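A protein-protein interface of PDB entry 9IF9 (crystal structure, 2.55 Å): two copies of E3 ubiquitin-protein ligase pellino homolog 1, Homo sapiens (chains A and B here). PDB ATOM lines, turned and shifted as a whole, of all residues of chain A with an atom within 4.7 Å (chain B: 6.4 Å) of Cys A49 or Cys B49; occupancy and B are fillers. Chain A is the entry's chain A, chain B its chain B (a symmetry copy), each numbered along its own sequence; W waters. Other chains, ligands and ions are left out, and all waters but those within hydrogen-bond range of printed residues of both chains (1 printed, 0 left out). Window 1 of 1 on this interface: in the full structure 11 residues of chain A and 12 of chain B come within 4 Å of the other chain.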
ATOM      1  N   ALA A  48      -7.302 -21.494  -2.666  1.00  0.00           N
ATOM      2  CA  ALA A  48      -6.040 -21.642  -1.964  1.00  0.00           C
ATOM      3  C   ALA A  48      -5.868 -23.115  -1.611  1.00  0.00           C
ATOM      4  O   ALA A  48      -6.771 -23.927  -1.821  1.00  0.00           O
ATOM      5  CB  ALA A  48      -6.009 -20.728  -0.734  1.00  0.00           C
ATOM      6  N   CYS A  49      -4.714 -23.476  -1.048  1.00  0.00           N
ATOM      7  CA  CYS A  49      -4.448 -24.887  -0.733  1.00  0.00           C
ATOM      8  C   CYS A  49      -4.922 -25.252   0.676  1.00  0.00           C
ATOM      9  O   CYS A  49      -4.156 -25.722   1.518  1.00  0.00           O
ATOM     10  CB  CYS A  49      -2.971 -25.224  -0.912  1.00  0.00           C
ATOM     11  SG  CYS A  49      -2.756 -26.828  -1.747  1.00  0.00           S
ATOM     12  N   THR A  50      -6.223 -25.073   0.902  1.00  0.00           N
ATOM     13  CA  THR A  50      -6.811 -25.483   2.169  1.00  0.00           C
ATOM     14  C   THR A  50      -6.797 -27.011   2.248  1.00  0.00           C
ATOM     15  O   THR A  50      -6.684 -27.687   1.227  1.00  0.00           O
ATOM     16  CB  THR A  50      -8.238 -24.951   2.309  1.00  0.00           C
ATOM     17  OG1 THR A  50      -9.165 -25.945   1.873  1.00  0.00           O
ATOM     18  CG2 THR A  50      -8.420 -23.716   1.423  1.00  0.00           C
ATOM     19  N   PRO A  51      -6.879 -27.588   3.449  1.00  0.00           N
ATOM     20  CA  PRO A  51      -6.874 -29.058   3.526  1.00  0.00           C
ATOM     21  C   PRO A  51      -7.977 -29.708   2.699  1.00  0.00           C
ATOM     22  O   PRO A  51      -7.807 -30.841   2.234  1.00  0.00           O
ATOM     23  CB  PRO A  51      -7.028 -29.324   5.028  1.00  0.00           C
ATOM     24  CG  PRO A  51      -7.544 -28.025   5.595  1.00  0.00           C
ATOM     25  CD  PRO A  51      -6.878 -26.978   4.789  1.00  0.00           C
ATOM     26  N   ALA A  53      -9.238 -28.575  -0.357  1.00  0.00           N
ATOM     27  CA  ALA A  53      -8.713 -28.628  -1.718  1.00  0.00           C
ATOM     28  C   ALA A  53      -7.629 -29.681  -1.828  1.00  0.00           C
ATOM     29  O   ALA A  53      -7.529 -30.382  -2.840  1.00  0.00           O
ATOM     30  CB  ALA A  53      -8.162 -27.265  -2.126  1.00  0.00           C
ATOM     31  N   ALA A  54      -6.805 -29.805  -0.792  1.00  0.00           N
ATOM     32  CA  ALA A  54      -5.729 -30.788  -0.802  1.00  0.00           C
ATOM     33  C   ALA A  54      -6.284 -32.203  -0.878  1.00  0.00           C
ATOM     34  O   ALA A  54      -5.766 -33.037  -1.626  1.00  0.00           O
ATOM     35  CB  ALA A  54      -4.853 -30.608   0.442  1.00  0.00           C
ATOM     36  N   ILE A  57      -7.627 -33.056  -4.592  1.00  0.00           N
ATOM     37  CA  ILE A  57      -6.601 -33.457  -5.554  1.00  0.00           C
ATOM     38  C   ILE A  57      -6.027 -34.813  -5.177  1.00  0.00           C
ATOM     39  O   ILE A  57      -5.885 -35.703  -6.018  1.00  0.00           O
ATOM     40  CB  ILE A  57      -5.491 -32.395  -5.661  1.00  0.00           C
ATOM     41  CG1 ILE A  57      -6.084 -31.031  -5.970  1.00  0.00           C
ATOM     42  CG2 ILE A  57      -4.430 -32.815  -6.680  1.00  0.00           C
ATOM     43  CD1 ILE A  57      -5.232 -29.906  -5.497  1.00  0.00           C
ATOM     44  N   THR A  74      -3.691 -21.381  -8.004  1.00  0.00           N
ATOM     45  CA  THR A  74      -4.371 -22.519  -8.611  1.00  0.00           C
ATOM     46  C   THR A  74      -5.782 -22.583  -8.048  1.00  0.00           C
ATOM     47  O   THR A  74      -5.979 -22.533  -6.829  1.00  0.00           O
ATOM     48  CB  THR A  74      -3.645 -23.848  -8.358  1.00  0.00           C
ATOM     49  OG1 THR A  74      -2.458 -23.905  -9.162  1.00  0.00           O
ATOM     50  CG2 THR A  74      -4.554 -25.041  -8.691  1.00  0.00           C
ATOM     51  N   VAL A  76      -8.885 -24.987  -7.625  1.00  0.00           N
ATOM     52  CA  VAL A  76      -9.217 -26.403  -7.605  1.00  0.00           C
ATOM     53  C   VAL A  76     -10.722 -26.481  -7.442  1.00  0.00           C
ATOM     54  O   VAL A  76     -11.286 -25.871  -6.521  1.00  0.00           O
ATOM     55  CB  VAL A  76      -8.479 -27.158  -6.486  1.00  0.00           C
ATOM     56  CG1 VAL A  76      -8.890 -28.610  -6.452  1.00  0.00           C
ATOM     57  CG2 VAL A  76      -6.987 -27.055  -6.695  1.00  0.00           C
ATOM     58  N   ILE B  47       3.844 -22.887  -3.322  1.00  0.00           N
ATOM     59  CA  ILE B  47       3.173 -21.596  -3.279  1.00  0.00           C
ATOM     60  C   ILE B  47       1.790 -21.630  -3.916  1.00  0.00           C
ATOM     61  O   ILE B  47       1.076 -20.616  -3.886  1.00  0.00           O
ATOM     62  CB  ILE B  47       4.050 -20.500  -3.915  1.00  0.00           C
ATOM     63  CG1 ILE B  47       4.340 -20.797  -5.373  1.00  0.00           C
ATOM     64  CG2 ILE B  47       5.372 -20.463  -3.232  1.00  0.00           C
ATOM     65  CD1 ILE B  47       4.624 -19.554  -6.172  1.00  0.00           C
ATOM     66  N   ALA B  48       1.376 -22.766  -4.466  1.00  0.00           N
ATOM     67  CA  ALA B  48       0.031 -22.885  -5.001  1.00  0.00           C
ATOM     68  C   ALA B  48      -0.389 -24.342  -4.916  1.00  0.00           C
ATOM     69  O   ALA B  48       0.452 -25.237  -4.837  1.00  0.00           O
ATOM     70  CB  ALA B  48      -0.043 -22.376  -6.443  1.00  0.00           C
ATOM     71  N   CYS B  49      -1.701 -24.581  -4.947  1.00  0.00           N
ATOM     72  CA  CYS B  49      -2.191 -25.941  -4.733  1.00  0.00           C
ATOM     73  C   CYS B  49      -1.803 -26.911  -5.848  1.00  0.00           C
ATOM     74  O   CYS B  49      -2.662 -27.505  -6.514  1.00  0.00           O
ATOM     75  CB  CYS B  49      -3.704 -25.956  -4.541  1.00  0.00           C
ATOM     76  SG  CYS B  49      -4.123 -27.148  -3.253  1.00  0.00           S
ATOM     77  N   THR B  50      -0.502 -27.097  -6.023  1.00  0.00           N
ATOM     78  CA  THR B  50       0.020 -28.100  -6.925  1.00  0.00           C
ATOM     79  C   THR B  50      -0.197 -29.494  -6.330  1.00  0.00           C
ATOM     80  O   THR B  50      -0.373 -29.634  -5.119  1.00  0.00           O
ATOM     81  CB  THR B  50       1.502 -27.844  -7.161  1.00  0.00           C
ATOM     82  OG1 THR B  50       2.221 -28.087  -5.950  1.00  0.00           O
ATOM     83  CG2 THR B  50       1.706 -26.391  -7.564  1.00  0.00           C
ATOM     84  N   PRO B  51      -0.198 -30.543  -7.162  1.00  0.00           N
ATOM     85  CA  PRO B  51      -0.519 -31.870  -6.621  1.00  0.00           C
ATOM     86  C   PRO B  51       0.446 -32.303  -5.546  1.00  0.00           C
ATOM     87  O   PRO B  51       0.034 -32.940  -4.566  1.00  0.00           O
ATOM     88  CB  PRO B  51      -0.449 -32.772  -7.858  1.00  0.00           C
ATOM     89  CG  PRO B  51      -0.628 -31.863  -8.997  1.00  0.00           C
ATOM     90  CD  PRO B  51       0.085 -30.618  -8.604  1.00  0.00           C
ATOM     91  N   GLN B  52       1.728 -31.953  -5.697  1.00  0.00           N
ATOM     92  CA  GLN B  52       2.679 -32.203  -4.621  1.00  0.00           C
ATOM     93  C   GLN B  52       2.308 -31.423  -3.373  1.00  0.00           C
ATOM     94  O   GLN B  52       2.323 -31.969  -2.264  1.00  0.00           O
ATOM     95  CB  GLN B  52       4.097 -31.858  -5.067  1.00  0.00           C
ATOM     96  CG  GLN B  52       5.129 -32.892  -4.631  1.00  0.00           C
ATOM     97  CD  GLN B  52       4.800 -34.324  -5.095  1.00  0.00           C
ATOM     98  OE1 GLN B  52       3.978 -34.536  -6.002  1.00  0.00           O
ATOM     99  NE2 GLN B  52       5.435 -35.316  -4.458  1.00  0.00           N
ATOM    100  N   ALA B  53       1.970 -30.143  -3.533  1.00  0.00           N
ATOM    101  CA  ALA B  53       1.516 -29.353  -2.391  1.00  0.00           C
ATOM    102  C   ALA B  53       0.322 -30.010  -1.714  1.00  0.00           C
ATOM    103  O   ALA B  53       0.213 -29.997  -0.487  1.00  0.00           O
ATOM    104  CB  ALA B  53       1.158 -27.939  -2.836  1.00  0.00           C
ATOM    105  N   ALA B  54      -0.580 -30.592  -2.508  1.00  0.00           N
ATOM    106  CA  ALA B  54      -1.737 -31.287  -1.958  1.00  0.00           C
ATOM    107  C   ALA B  54      -1.312 -32.564  -1.256  1.00  0.00           C
ATOM    108  O   ALA B  54      -1.863 -32.904  -0.202  1.00  0.00           O
ATOM    109  CB  ALA B  54      -2.742 -31.595  -3.071  1.00  0.00           C
ATOM    110  N   ILE B  57      -0.222 -32.071   2.381  1.00  0.00           N
ATOM    111  CA  ILE B  57      -1.219 -31.819   3.424  1.00  0.00           C
ATOM    112  C   ILE B  57      -2.082 -33.052   3.698  1.00  0.00           C
ATOM    113  O   ILE B  57      -2.407 -33.346   4.854  1.00  0.00           O
ATOM    114  CB  ILE B  57      -2.089 -30.584   3.072  1.00  0.00           C
ATOM    115  CG1 ILE B  57      -1.241 -29.330   2.881  1.00  0.00           C
ATOM    116  CG2 ILE B  57      -3.107 -30.313   4.147  1.00  0.00           C
ATOM    117  CD1 ILE B  57      -1.979 -28.256   2.184  1.00  0.00           C
ATOM    118  N   SER B  66       1.317 -24.888   6.913  1.00  0.00           N
ATOM    119  CA  SER B  66       0.530 -24.132   5.941  1.00  0.00           C
ATOM    120  C   SER B  66       0.398 -22.683   6.398  1.00  0.00           C
ATOM    121  O   SER B  66      -0.216 -22.411   7.435  1.00  0.00           O
ATOM    122  CB  SER B  66      -0.853 -24.760   5.763  1.00  0.00           C
ATOM    123  OG  SER B  66      -0.762 -26.173   5.735  1.00  0.00           O
ATOM    124  N   ALA B  72      -6.488 -16.115  -1.410  1.00  0.00           N
ATOM    125  CA  ALA B  72      -6.111 -16.803  -2.641  1.00  0.00           C
ATOM    126  C   ALA B  72      -4.827 -17.619  -2.534  1.00  0.00           C
ATOM    127  O   ALA B  72      -4.484 -18.324  -3.497  1.00  0.00           O
ATOM    128  CB  ALA B  72      -5.963 -15.800  -3.792  1.00  0.00           C
ATOM    129  N   GLN B  73      -4.119 -17.560  -1.404  1.00  0.00           N
ATOM    130  CA  GLN B  73      -2.832 -18.230  -1.284  1.00  0.00           C
ATOM    131  C   GLN B  73      -2.631 -18.772   0.118  1.00  0.00           C
ATOM    132  O   GLN B  73      -2.808 -18.038   1.091  1.00  0.00           O
ATOM    133  CB  GLN B  73      -1.679 -17.284  -1.619  1.00  0.00           C
ATOM    134  CG  GLN B  73      -0.346 -17.964  -1.452  1.00  0.00           C
ATOM    135  CD  GLN B  73       0.714 -17.370  -2.332  1.00  0.00           C
ATOM    136  OE1 GLN B  73       0.947 -16.158  -2.306  1.00  0.00           O
ATOM    137  NE2 GLN B  73       1.354 -18.217  -3.142  1.00  0.00           N
ATOM    138  N   THR B  74      -2.268 -20.053   0.214  1.00  0.00           N
ATOM    139  CA  THR B  74      -1.644 -20.594   1.410  1.00  0.00           C
ATOM    140  C   THR B  74      -0.394 -21.344   0.980  1.00  0.00           C
ATOM    141  O   THR B  74      -0.407 -22.050  -0.028  1.00  0.00           O
ATOM    142  CB  THR B  74      -2.572 -21.540   2.249  1.00  0.00           C
ATOM    143  OG1 THR B  74      -2.219 -22.900   2.003  1.00  0.00           O
ATOM    144  CG2 THR B  74      -4.076 -21.314   2.005  1.00  0.00           C
ATOM    145  N   VAL B  75       0.690 -21.180   1.739  1.00  0.00           N
ATOM    146  CA  VAL B  75       2.006 -21.709   1.376  1.00  0.00           C
ATOM    147  C   VAL B  75       2.308 -22.942   2.214  1.00  0.00           C
ATOM    148  O   VAL B  75       2.301 -22.876   3.450  1.00  0.00           O
ATOM    149  CB  VAL B  75       3.108 -20.661   1.587  1.00  0.00           C
ATOM    150  CG1 VAL B  75       4.473 -21.328   1.525  1.00  0.00           C
ATOM    151  CG2 VAL B  75       2.986 -19.538   0.577  1.00  0.00           C
ATOM    152  N   VAL B  76       2.649 -24.041   1.552  1.00  0.00           N
ATOM    153  CA  VAL B  76       2.843 -25.323   2.216  1.00  0.00           C
ATOM    154  C   VAL B  76       4.337 -25.650   2.223  1.00  0.00           C
ATOM    155  O   VAL B  76       4.922 -26.010   1.191  1.00  0.00           O
ATOM    156  CB  VAL B  76       1.999 -26.423   1.559  1.00  0.00           C
ATOM    157  CG1 VAL B  76       2.167 -27.734   2.279  1.00  0.00           C
ATOM    158  CG2 VAL B  76       0.554 -26.011   1.623  1.00  0.00           C
HETATM  159  O   HOH W   1      -3.407 -26.207   4.131  1.00  0.00           O
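The side-chain sulfur (SG) of Cys A49 is disulfide-bonded to the side-chain sulfur (SG) of Cys B49, 2.1 Å away. The backbone carbonyl oxygen (O) of Cys A49 lies within hydrogen-bond range of the side-chain hydroxyl (OG1) of Thr B74 (3.5 Å).
Cys A49 touches three residues of chain B. Cys B49 touches just these residues of chain A: Cys A49 (2.1 Å), Ile A57 (3.7 Å) and Thr A74 (3.8 Å). Of the printed residues of chain A, Ala B72 touches Ala A48 (3.8 Å). Of the printed residues of chain B, Ala A54 touches Ala B54 (3.6 Å) and Ile B57 (3.8 Å). Of the printed residues of chain B, Ile A57 touches Cys B49 (3.7 Å) and Ala B54 (3.9 Å). Of the printed residues of chain A, Ile B57 touches Cys A49 (3.4 Å) and Ala A54 (3.8 Å). Of the printed residues of chain A, Gln B73 touches Ala A48. Ser B66 touches none of the printed residues of chain A. The nearest residue of chain B that does not touch Cys A49 is Ala B53 (4.2 Å). The nearest printed residue of chain A that does not touch Gln B73 is Cys A49 (5.3 Å).
Ala A48 touches Thr B74, and with the chains exchanged Thr A74 touches Ala B48. Cys A49 touches Ile B57, and with the chains exchanged Ile A57 touches Cys B49. Cys A49 touches Thr B74, and with the chains exchanged Thr A74 touches Cys B49. Ala B54 touches its own counterpart, Ala A54. Positions printed for both chains: 48, 49, 50, 51, 53, 54, 57, 74 and 76.
The backbone carbonyl oxygen (O) of Ile B47 lies within hydrogen-bond range of the side-chain amide nitrogen (NE2) of Gln B73, 2.5 Å away.
Water W1 lies within hydrogen-bond range of the backbone carbonyl oxygen of Cys A49 and the side-chain hydroxyl of Ser B66.
Hydrophobic or aromatic side chains of chain B that line the printed part of chain A: Ala B48, Ala B54 and Ile B57. Printed residues of chain A that touch a printed residue of chain B: Ala A48, Cys A49, Ala A54, Ile A57 and Thr A74. Among the printed residues, no Asp or Glu carboxylate lies within 4 Å of a Lys or Arg side-chain nitrogen of the other chain.
CB of Ala A48 touches C of Ala B72, at 3.8 Å. Ala A48 touches Gln B73 (CB to N, 3.7 Å). CB of Ala A48 touches CG2 of Thr B74 (3.4 Å). Cys A49 touches Ile B57. CB of Ala B54 touches O of Ala A54, 3.6 Å away. Ile B57 touches Ala A54. Ile A57 touches Cys B49. CB of Ile A57 touches CB of Ala B54, 3.9 Å away. OG1 of Thr A74 touches CB of Ala B48, at 3.9 Å. O of Cys B49 touches CG2 of Thr A74 (3.8 Å).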
